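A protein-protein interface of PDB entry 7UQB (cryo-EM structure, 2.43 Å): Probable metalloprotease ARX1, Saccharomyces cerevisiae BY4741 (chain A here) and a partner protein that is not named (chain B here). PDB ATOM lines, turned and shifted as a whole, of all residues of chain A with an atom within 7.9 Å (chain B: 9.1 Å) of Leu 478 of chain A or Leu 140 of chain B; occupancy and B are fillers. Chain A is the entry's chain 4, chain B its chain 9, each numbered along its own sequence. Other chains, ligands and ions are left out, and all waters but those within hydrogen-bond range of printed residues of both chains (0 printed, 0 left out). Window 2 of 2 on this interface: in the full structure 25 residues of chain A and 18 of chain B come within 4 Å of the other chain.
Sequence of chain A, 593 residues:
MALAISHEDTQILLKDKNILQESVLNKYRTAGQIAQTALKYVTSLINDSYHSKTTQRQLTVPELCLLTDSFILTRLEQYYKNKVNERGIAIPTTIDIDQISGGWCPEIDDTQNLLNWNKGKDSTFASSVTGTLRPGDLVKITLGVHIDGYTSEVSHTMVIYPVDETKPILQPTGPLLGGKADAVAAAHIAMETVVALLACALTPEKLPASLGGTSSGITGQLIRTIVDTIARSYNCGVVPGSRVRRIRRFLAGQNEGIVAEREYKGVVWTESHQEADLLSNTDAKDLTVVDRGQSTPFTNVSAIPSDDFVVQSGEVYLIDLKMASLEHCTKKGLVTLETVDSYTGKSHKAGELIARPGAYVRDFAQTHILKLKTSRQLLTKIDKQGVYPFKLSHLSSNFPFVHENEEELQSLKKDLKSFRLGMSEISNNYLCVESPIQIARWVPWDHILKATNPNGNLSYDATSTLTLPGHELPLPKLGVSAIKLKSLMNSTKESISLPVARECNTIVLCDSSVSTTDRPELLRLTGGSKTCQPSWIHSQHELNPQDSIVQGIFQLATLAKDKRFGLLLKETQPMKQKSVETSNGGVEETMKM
The backbone carbonyl oxygen of Leu 449 of chain A is in hydrogen-bond range of the side-chain amino group of Lys 144 of chain B, 2.6 Å away.
OE2 of Glu 275 of chain A sits at hydrogen-bond distance from N of Leu 478 of chain A, 3.0 Å away.
Leu 278 of chain A touches Leu 147 of chain B (CD2 to CG, 3.98 Å). CB of Ala 146 of chain B touches CD1 of Leu 279 of chain A (3.9 Å). CD1 of Leu 279 of chain A touches CD1 of Leu 147 of chain B (3.6 Å). Leu 147 of chain B touches Leu 449 of chain A. CE3 of Trp 148 of chain B touches CD1 of Leu 449 of chain A, at 3.6 Å. Leu 140 of chain B touches Leu 478 of chain A (CD1 to O, 3.7 Å). Leu 478 of chain A touches Val 143 of chain B. Leu 478 of chain A touches Lys 144 of chain B. Leu 478 of chain A touches Leu 147 of chain B.
Ile 448 of chain A touches none of the printed residues of chain B. Of the printed residues of chain B, Leu 478 of chain A touches Leu 140 (3.7 Å), Val 143 (3.9 Å), Lys 144 (3.9 Å) and Leu 147 (3.7 Å). Printed residues of chain A within 4 Å of Val 143 of chain B: Leu 478. Of the printed residues of chain A, Leu 147 of chain B touches Leu 278 (3.98 Å), Leu 279 (3.6 Å), Leu 449 (3.7 Å) and Leu 478 (3.7 Å).
Of the 11 printed residues of chain B, 6 touch a printed residue of chain A. Printed residues of chain B that touch a printed residue of chain A: Leu 140, Val 143, Lys 144, Ala 146, Leu 147 and Trp 148. Hydrophobic or aromatic side chains of chain A that line the printed part of chain B: Leu 278, Leu 279, Leu 449 and Leu 478. Among the printed residues, no Asp or Glu carboxylate lies within 4 Å of a Lys or Arg side-chain nitrogen of the other chain.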
ATOM      1  N   GLU A 275       4.744 -23.777   3.888  1.00  0.00           N
ATOM      2  CA  GLU A 275       4.765 -24.852   4.876  1.00  0.00           C
ATOM      3  C   GLU A 275       4.801 -26.219   4.204  1.00  0.00           C
ATOM      4  O   GLU A 275       5.555 -27.106   4.621  1.00  0.00           O
ATOM      5  CB  GLU A 275       3.543 -24.727   5.784  1.00  0.00           C
ATOM      6  CG  GLU A 275       3.448 -25.754   6.894  1.00  0.00           C
ATOM      7  CD  GLU A 275       2.061 -25.798   7.507  1.00  0.00           C
ATOM      8  OE1 GLU A 275       1.076 -25.673   6.751  1.00  0.00           O
ATOM      9  OE2 GLU A 275       1.955 -25.947   8.740  1.00  0.00           O
ATOM     10  N   LEU A 278       8.257 -26.808   2.718  1.00  0.00           N
ATOM     11  CA  LEU A 278       9.195 -27.153   3.782  1.00  0.00           C
ATOM     12  C   LEU A 278       8.977 -28.583   4.264  1.00  0.00           C
ATOM     13  O   LEU A 278       9.938 -29.295   4.574  1.00  0.00           O
ATOM     14  CB  LEU A 278       9.054 -26.169   4.942  1.00  0.00           C
ATOM     15  CG  LEU A 278      10.006 -26.360   6.122  1.00  0.00           C
ATOM     16  CD1 LEU A 278      11.401 -25.870   5.771  1.00  0.00           C
ATOM     17  CD2 LEU A 278       9.481 -25.662   7.366  1.00  0.00           C
ATOM     18  N   LEU A 279       7.720 -29.021   4.326  1.00  0.00           N
ATOM     19  CA  LEU A 279       7.382 -30.340   4.847  1.00  0.00           C
ATOM     20  C   LEU A 279       7.496 -31.448   3.804  1.00  0.00           C
ATOM     21  O   LEU A 279       7.390 -32.625   4.163  1.00  0.00           O
ATOM     22  CB  LEU A 279       5.964 -30.300   5.426  1.00  0.00           C
ATOM     23  CG  LEU A 279       5.533 -31.367   6.431  1.00  0.00           C
ATOM     24  CD1 LEU A 279       6.707 -31.796   7.297  1.00  0.00           C
ATOM     25  CD2 LEU A 279       4.400 -30.837   7.291  1.00  0.00           C
ATOM     26  N   LEU A 334       9.626 -18.122   7.529  1.00  0.00           N
ATOM     27  CA  LEU A 334       8.393 -17.996   6.765  1.00  0.00           C
ATOM     28  C   LEU A 334       8.180 -16.545   6.354  1.00  0.00           C
ATOM     29  O   LEU A 334       8.348 -15.629   7.166  1.00  0.00           O
ATOM     30  CB  LEU A 334       7.196 -18.486   7.587  1.00  0.00           C
ATOM     31  CG  LEU A 334       5.789 -18.334   7.006  1.00  0.00           C
ATOM     32  CD1 LEU A 334       5.485 -19.437   6.013  1.00  0.00           C
ATOM     33  CD2 LEU A 334       4.756 -18.311   8.121  1.00  0.00           C
ATOM     34  N   TRP A 445      11.201 -20.150  11.761  1.00  0.00           N
ATOM     35  CA  TRP A 445      10.386 -21.331  12.037  1.00  0.00           C
ATOM     36  C   TRP A 445      10.523 -21.809  13.478  1.00  0.00           C
ATOM     37  O   TRP A 445       9.575 -22.386  14.025  1.00  0.00           O
ATOM     38  CB  TRP A 445      10.755 -22.465  11.079  1.00  0.00           C
ATOM     39  CG  TRP A 445      10.160 -22.341   9.709  1.00  0.00           C
ATOM     40  CD1 TRP A 445      10.823 -22.075   8.549  1.00  0.00           C
ATOM     41  CD2 TRP A 445       8.779 -22.487   9.356  1.00  0.00           C
ATOM     42  NE1 TRP A 445       9.945 -22.041   7.496  1.00  0.00           N
ATOM     43  CE2 TRP A 445       8.682 -22.292   7.963  1.00  0.00           C
ATOM     44  CE3 TRP A 445       7.615 -22.758  10.080  1.00  0.00           C
ATOM     45  CZ2 TRP A 445       7.469 -22.362   7.283  1.00  0.00           C
ATOM     46  CZ3 TRP A 445       6.411 -22.827   9.403  1.00  0.00           C
ATOM     47  CH2 TRP A 445       6.347 -22.630   8.019  1.00  0.00           C
ATOM     48  N   ILE A 448       8.074 -20.023  15.739  1.00  0.00           N
ATOM     49  CA  ILE A 448       6.732 -20.534  15.475  1.00  0.00           C
ATOM     50  C   ILE A 448       6.528 -21.878  16.162  1.00  0.00           C
ATOM     51  O   ILE A 448       5.489 -22.120  16.789  1.00  0.00           O
ATOM     52  CB  ILE A 448       6.493 -20.639  13.956  1.00  0.00           C
ATOM     53  CG1 ILE A 448       6.628 -19.267  13.293  1.00  0.00           C
ATOM     54  CG2 ILE A 448       5.130 -21.249  13.663  1.00  0.00           C
ATOM     55  CD1 ILE A 448       6.452 -19.294  11.789  1.00  0.00           C
ATOM     56  N   LEU A 449       7.517 -22.769  16.057  1.00  0.00           N
ATOM     57  CA  LEU A 449       7.395 -24.088  16.674  1.00  0.00           C
ATOM     58  C   LEU A 449       7.364 -23.997  18.196  1.00  0.00           C
ATOM     59  O   LEU A 449       6.575 -24.693  18.846  1.00  0.00           O
ATOM     60  CB  LEU A 449       8.534 -24.992  16.207  1.00  0.00           C
ATOM     61  CG  LEU A 449       8.495 -25.393  14.731  1.00  0.00           C
ATOM     62  CD1 LEU A 449       9.686 -26.265  14.375  1.00  0.00           C
ATOM     63  CD2 LEU A 449       7.190 -26.099  14.399  1.00  0.00           C
ATOM     64  N   ALA A 451       6.293 -21.527  19.951  1.00  0.00           N
ATOM     65  CA  ALA A 451       5.108 -20.821  20.412  1.00  0.00           C
ATOM     66  C   ALA A 451       3.964 -21.784  20.714  1.00  0.00           C
ATOM     67  O   ALA A 451       3.895 -22.895  20.183  1.00  0.00           O
ATOM     68  CB  ALA A 451       4.662 -19.807  19.368  1.00  0.00           C
ATOM     69  N   ASN A 453      -0.273 -22.025  20.840  1.00  0.00           N
ATOM     70  CA  ASN A 453      -1.590 -21.479  20.512  1.00  0.00           C
ATOM     71  C   ASN A 453      -2.652 -22.303  21.227  1.00  0.00           C
ATOM     72  O   ASN A 453      -2.940 -23.440  20.815  1.00  0.00           O
ATOM     73  CB  ASN A 453      -1.832 -21.463  19.002  1.00  0.00           C
ATOM     74  CG  ASN A 453      -1.363 -22.729  18.318  1.00  0.00           C
ATOM     75  OD1 ASN A 453      -0.487 -23.431  18.821  1.00  0.00           O
ATOM     76  ND2 ASN A 453      -1.944 -23.026  17.162  1.00  0.00           N
ATOM     77  N   GLY A 456      -5.708 -23.283  18.671  1.00  0.00           N
ATOM     78  CA  GLY A 456      -5.545 -24.107  17.483  1.00  0.00           C
ATOM     79  C   GLY A 456      -6.235 -23.476  16.290  1.00  0.00           C
ATOM     80  O   GLY A 456      -6.110 -22.273  16.038  1.00  0.00           O
ATOM     81  N   ASN A 457      -6.978 -24.296  15.543  1.00  0.00           N
ATOM     82  CA  ASN A 457      -7.708 -23.811  14.375  1.00  0.00           C
ATOM     83  C   ASN A 457      -8.846 -22.867  14.737  1.00  0.00           C
ATOM     84  O   ASN A 457      -9.291 -22.101  13.876  1.00  0.00           O
ATOM     85  CB  ASN A 457      -8.283 -24.985  13.581  1.00  0.00           C
ATOM     86  CG  ASN A 457      -7.215 -25.904  13.039  1.00  0.00           C
ATOM     87  OD1 ASN A 457      -6.118 -25.466  12.703  1.00  0.00           O
ATOM     88  ND2 ASN A 457      -7.536 -27.188  12.946  1.00  0.00           N
ATOM     89  N   LEU A 473      -6.355 -19.507   7.433  1.00  0.00           N
ATOM     90  CA  LEU A 473      -5.384 -20.398   8.067  1.00  0.00           C
ATOM     91  C   LEU A 473      -4.080 -20.338   7.283  1.00  0.00           C
ATOM     92  O   LEU A 473      -3.909 -21.057   6.287  1.00  0.00           O
ATOM     93  CB  LEU A 473      -5.907 -21.831   8.141  1.00  0.00           C
ATOM     94  CG  LEU A 473      -6.606 -22.262   9.430  1.00  0.00           C
ATOM     95  CD1 LEU A 473      -7.028 -23.718   9.343  1.00  0.00           C
ATOM     96  CD2 LEU A 473      -5.701 -22.039  10.629  1.00  0.00           C
ATOM     97  N   PRO A 474      -3.131 -19.490   7.692  1.00  0.00           N
ATOM     98  CA  PRO A 474      -1.845 -19.444   6.980  1.00  0.00           C
ATOM     99  C   PRO A 474      -1.000 -20.693   7.173  1.00  0.00           C
ATOM    100  O   PRO A 474      -0.164 -20.994   6.314  1.00  0.00           O
ATOM    101  CB  PRO A 474      -1.166 -18.200   7.566  1.00  0.00           C
ATOM    102  CG  PRO A 474      -1.774 -18.042   8.915  1.00  0.00           C
ATOM    103  CD  PRO A 474      -3.196 -18.511   8.790  1.00  0.00           C
ATOM    104  N   LEU A 475      -1.187 -21.427   8.269  1.00  0.00           N
ATOM    105  CA  LEU A 475      -0.442 -22.656   8.545  1.00  0.00           C
ATOM    106  C   LEU A 475      -1.431 -23.752   8.923  1.00  0.00           C
ATOM    107  O   LEU A 475      -1.621 -24.050  10.110  1.00  0.00           O
ATOM    108  CB  LEU A 475       0.596 -22.437   9.646  1.00  0.00           C
ATOM    109  CG  LEU A 475       1.735 -21.467   9.320  1.00  0.00           C
ATOM    110  CD1 LEU A 475       2.589 -21.201  10.548  1.00  0.00           C
ATOM    111  CD2 LEU A 475       2.585 -22.008   8.185  1.00  0.00           C
ATOM    112  N   PRO A 476      -2.092 -24.364   7.933  1.00  0.00           N
ATOM    113  CA  PRO A 476      -3.107 -25.386   8.248  1.00  0.00           C
ATOM    114  C   PRO A 476      -2.555 -26.616   8.951  1.00  0.00           C
ATOM    115  O   PRO A 476      -3.229 -27.178   9.821  1.00  0.00           O
ATOM    116  CB  PRO A 476      -3.685 -25.739   6.868  1.00  0.00           C
ATOM    117  CG  PRO A 476      -3.280 -24.615   5.966  1.00  0.00           C
ATOM    118  CD  PRO A 476      -1.965 -24.143   6.485  1.00  0.00           C
ATOM    119  N   LYS A 477      -1.344 -27.052   8.597  1.00  0.00           N
ATOM    120  CA  LYS A 477      -0.798 -28.271   9.184  1.00  0.00           C
ATOM    121  C   LYS A 477      -0.327 -28.057  10.616  1.00  0.00           C
ATOM    122  O   LYS A 477      -0.407 -28.981  11.432  1.00  0.00           O
ATOM    123  CB  LYS A 477       0.347 -28.802   8.320  1.00  0.00           C
ATOM    124  CG  LYS A 477      -0.097 -29.276   6.948  1.00  0.00           C
ATOM    125  CD  LYS A 477       1.087 -29.660   6.080  1.00  0.00           C
ATOM    126  CE  LYS A 477       0.631 -30.320   4.791  1.00  0.00           C
ATOM    127  NZ  LYS A 477      -0.259 -29.434   3.993  1.00  0.00           N
ATOM    128  N   LEU A 478       0.168 -26.864  10.937  1.00  0.00           N
ATOM    129  CA  LEU A 478       0.558 -26.527  12.297  1.00  0.00           C
ATOM    130  C   LEU A 478      -0.604 -26.028  13.143  1.00  0.00           C
ATOM    131  O   LEU A 478      -0.435 -25.850  14.355  1.00  0.00           O
ATOM    132  CB  LEU A 478       1.661 -25.464  12.285  1.00  0.00           C
ATOM    133  CG  LEU A 478       3.049 -25.912  11.835  1.00  0.00           C
ATOM    134  CD1 LEU A 478       3.981 -24.719  11.735  1.00  0.00           C
ATOM    135  CD2 LEU A 478       3.605 -26.956  12.791  1.00  0.00           C
ATOM    136  N   GLY A 479      -1.770 -25.809  12.545  1.00  0.00           N
ATOM    137  CA  GLY A 479      -2.914 -25.288  13.274  1.00  0.00           C
ATOM    138  C   GLY A 479      -2.742 -23.870  13.777  1.00  0.00           C
ATOM    139  O   GLY A 479      -3.103 -23.579  14.925  1.00  0.00           O
ATOM    140  N   VAL A 480      -2.205 -22.980  12.949  1.00  0.00           N
ATOM    141  CA  VAL A 480      -1.905 -21.609  13.343  1.00  0.00           C
ATOM    142  C   VAL A 480      -2.754 -20.669  12.499  1.00  0.00           C
ATOM    143  O   VAL A 480      -2.690 -20.704  11.264  1.00  0.00           O
ATOM    144  CB  VAL A 480      -0.410 -21.288  13.190  1.00  0.00           C
ATOM    145  CG1 VAL A 480      -0.160 -19.803  13.401  1.00  0.00           C
ATOM    146  CG2 VAL A 480       0.407 -22.114  14.170  1.00  0.00           C
ATOM    147  N   SER A 481      -3.536 -19.824  13.163  1.00  0.00           N
ATOM    148  CA  SER A 481      -4.393 -18.867  12.485  1.00  0.00           C
ATOM    149  C   SER A 481      -3.635 -17.574  12.188  1.00  0.00           C
ATOM    150  O   SER A 481      -2.498 -17.374  12.618  1.00  0.00           O
ATOM    151  CB  SER A 481      -5.638 -18.577  13.322  1.00  0.00           C
ATOM    152  OG  SER A 481      -5.298 -18.008  14.574  1.00  0.00           O
ATOM    153  N   SER B 138       0.549 -38.273  18.378  1.00  0.00           N
ATOM    154  CA  SER B 138      -0.130 -37.040  17.993  1.00  0.00           C
ATOM    155  C   SER B 138       0.374 -36.543  16.642  1.00  0.00           C
ATOM    156  O   SER B 138       1.578 -36.359  16.448  1.00  0.00           O
ATOM    157  CB  SER B 138       0.063 -35.964  19.063  1.00  0.00           C
ATOM    158  OG  SER B 138      -0.627 -34.776  18.722  1.00  0.00           O
ATOM    159  N   SER B 139      -0.564 -36.331  15.714  1.00  0.00           N
ATOM    160  CA  SER B 139      -0.201 -35.920  14.361  1.00  0.00           C
ATOM    161  C   SER B 139       0.454 -34.545  14.353  1.00  0.00           C
ATOM    162  O   SER B 139       1.408 -34.309  13.603  1.00  0.00           O
ATOM    163  CB  SER B 139      -1.438 -35.932  13.463  1.00  0.00           C
ATOM    164  OG  SER B 139      -1.105 -35.603  12.125  1.00  0.00           O
ATOM    165  N   LEU B 140      -0.047 -33.625  15.182  1.00  0.00           N
ATOM    166  CA  LEU B 140       0.577 -32.310  15.300  1.00  0.00           C
ATOM    167  C   LEU B 140       2.003 -32.420  15.823  1.00  0.00           C
ATOM    168  O   LEU B 140       2.910 -31.737  15.330  1.00  0.00           O
ATOM    169  CB  LEU B 140      -0.264 -31.419  16.214  1.00  0.00           C
ATOM    170  CG  LEU B 140       0.415 -30.176  16.791  1.00  0.00           C
ATOM    171  CD1 LEU B 140       0.684 -29.143  15.706  1.00  0.00           C
ATOM    172  CD2 LEU B 140      -0.419 -29.587  17.918  1.00  0.00           C
ATOM    173  N   THR B 141       2.218 -33.279  16.823  1.00  0.00           N
ATOM    174  CA  THR B 141       3.559 -33.477  17.360  1.00  0.00           C
ATOM    175  C   THR B 141       4.493 -34.067  16.310  1.00  0.00           C
ATOM    176  O   THR B 141       5.650 -33.651  16.199  1.00  0.00           O
ATOM    177  CB  THR B 141       3.501 -34.375  18.596  1.00  0.00           C
ATOM    178  OG1 THR B 141       2.543 -33.846  19.522  1.00  0.00           O
ATOM    179  CG2 THR B 141       4.860 -34.444  19.273  1.00  0.00           C
ATOM    180  N   LEU B 142       4.004 -35.032  15.525  1.00  0.00           N
ATOM    181  CA  LEU B 142       4.824 -35.609  14.462  1.00  0.00           C
ATOM    182  C   LEU B 142       5.159 -34.573  13.396  1.00  0.00           C
ATOM    183  O   LEU B 142       6.282 -34.549  12.874  1.00  0.00           O
ATOM    184  CB  LEU B 142       4.112 -36.813  13.841  1.00  0.00           C
ATOM    185  CG  LEU B 142       3.971 -38.055  14.725  1.00  0.00           C
ATOM    186  CD1 LEU B 142       3.271 -39.175  13.969  1.00  0.00           C
ATOM    187  CD2 LEU B 142       5.330 -38.513  15.226  1.00  0.00           C
ATOM    188  N   VAL B 143       4.196 -33.710  13.061  1.00  0.00           N
ATOM    189  CA  VAL B 143       4.445 -32.636  12.101  1.00  0.00           C
ATOM    190  C   VAL B 143       5.515 -31.686  12.627  1.00  0.00           C
ATOM    191  O   VAL B 143       6.427 -31.287  11.892  1.00  0.00           O
ATOM    192  CB  VAL B 143       3.131 -31.898  11.778  1.00  0.00           C
ATOM    193  CG1 VAL B 143       3.407 -30.532  11.170  1.00  0.00           C
ATOM    194  CG2 VAL B 143       2.272 -32.731  10.836  1.00  0.00           C
ATOM    195  N   LYS B 144       5.425 -31.316  13.908  1.00  0.00           N
ATOM    196  CA  LYS B 144       6.422 -30.423  14.494  1.00  0.00           C
ATOM    197  C   LYS B 144       7.801 -31.074  14.534  1.00  0.00           C
ATOM    198  O   LYS B 144       8.814 -30.408  14.294  1.00  0.00           O
ATOM    199  CB  LYS B 144       5.987 -29.991  15.894  1.00  0.00           C
ATOM    200  CG  LYS B 144       4.780 -29.063  15.909  1.00  0.00           C
ATOM    201  CD  LYS B 144       4.291 -28.806  17.325  1.00  0.00           C
ATOM    202  CE  LYS B 144       5.207 -27.858  18.074  1.00  0.00           C
ATOM    203  NZ  LYS B 144       5.103 -26.470  17.551  1.00  0.00           N
ATOM    204  N   GLU B 145       7.861 -32.373  14.842  1.00  0.00           N
ATOM    205  CA  GLU B 145       9.144 -33.073  14.847  1.00  0.00           C
ATOM    206  C   GLU B 145       9.752 -33.130  13.451  1.00  0.00           C
ATOM    207  O   GLU B 145      10.962 -32.933  13.287  1.00  0.00           O
ATOM    208  CB  GLU B 145       8.982 -34.482  15.418  1.00  0.00           C
ATOM    209  CG  GLU B 145       8.608 -34.528  16.892  1.00  0.00           C
ATOM    210  CD  GLU B 145       9.540 -33.707  17.763  1.00  0.00           C
ATOM    211  OE1 GLU B 145      10.771 -33.793  17.575  1.00  0.00           O
ATOM    212  OE2 GLU B 145       9.036 -32.972  18.639  1.00  0.00           O
ATOM    213  N   ALA B 146       8.928 -33.392  12.431  1.00  0.00           N
ATOM    214  CA  ALA B 146       9.427 -33.394  11.059  1.00  0.00           C
ATOM    215  C   ALA B 146       9.903 -32.008  10.638  1.00  0.00           C
ATOM    216  O   ALA B 146      10.914 -31.878   9.937  1.00  0.00           O
ATOM    217  CB  ALA B 146       8.345 -33.903  10.109  1.00  0.00           C
ATOM    218  N   LEU B 147       9.182 -30.961  11.051  1.00  0.00           N
ATOM    219  CA  LEU B 147       9.608 -29.596  10.755  1.00  0.00           C
ATOM    220  C   LEU B 147      10.940 -29.274  11.422  1.00  0.00           C
ATOM    221  O   LEU B 147      11.813 -28.646  10.813  1.00  0.00           O
ATOM    222  CB  LEU B 147       8.538 -28.601  11.203  1.00  0.00           C
ATOM    223  CG  LEU B 147       7.704 -27.904  10.127  1.00  0.00           C
ATOM    224  CD1 LEU B 147       6.773 -28.880   9.445  1.00  0.00           C
ATOM    225  CD2 LEU B 147       6.918 -26.753  10.729  1.00  0.00           C
ATOM    226  N   TRP B 148      11.112 -29.692  12.678  1.00  0.00           N
ATOM    227  CA  TRP B 148      12.381 -29.465  13.359  1.00  0.00           C
ATOM    228  C   TRP B 148      13.508 -30.236  12.683  1.00  0.00           C
ATOM    229  O   TRP B 148      14.638 -29.742  12.587  1.00  0.00           O
ATOM    230  CB  TRP B 148      12.272 -29.853  14.832  1.00  0.00           C
ATOM    231  CG  TRP B 148      13.419 -29.354  15.643  1.00  0.00           C
ATOM    232  CD1 TRP B 148      14.555 -30.039  15.970  1.00  0.00           C
ATOM    233  CD2 TRP B 148      13.556 -28.051  16.220  1.00  0.00           C
ATOM    234  NE1 TRP B 148      15.386 -29.242  16.721  1.00  0.00           N
ATOM    235  CE2 TRP B 148      14.796 -28.017  16.888  1.00  0.00           C
ATOM    236  CE3 TRP B 148      12.748 -26.909  16.239  1.00  0.00           C
ATOM    237  CZ2 TRP B 148      15.246 -26.889  17.569  1.00  0.00           C
ATOM    238  CZ3 TRP B 148      13.197 -25.790  16.913  1.00  0.00           C
ATOM    239  CH2 TRP B 148      14.434 -25.788  17.569  1.00  0.00           C
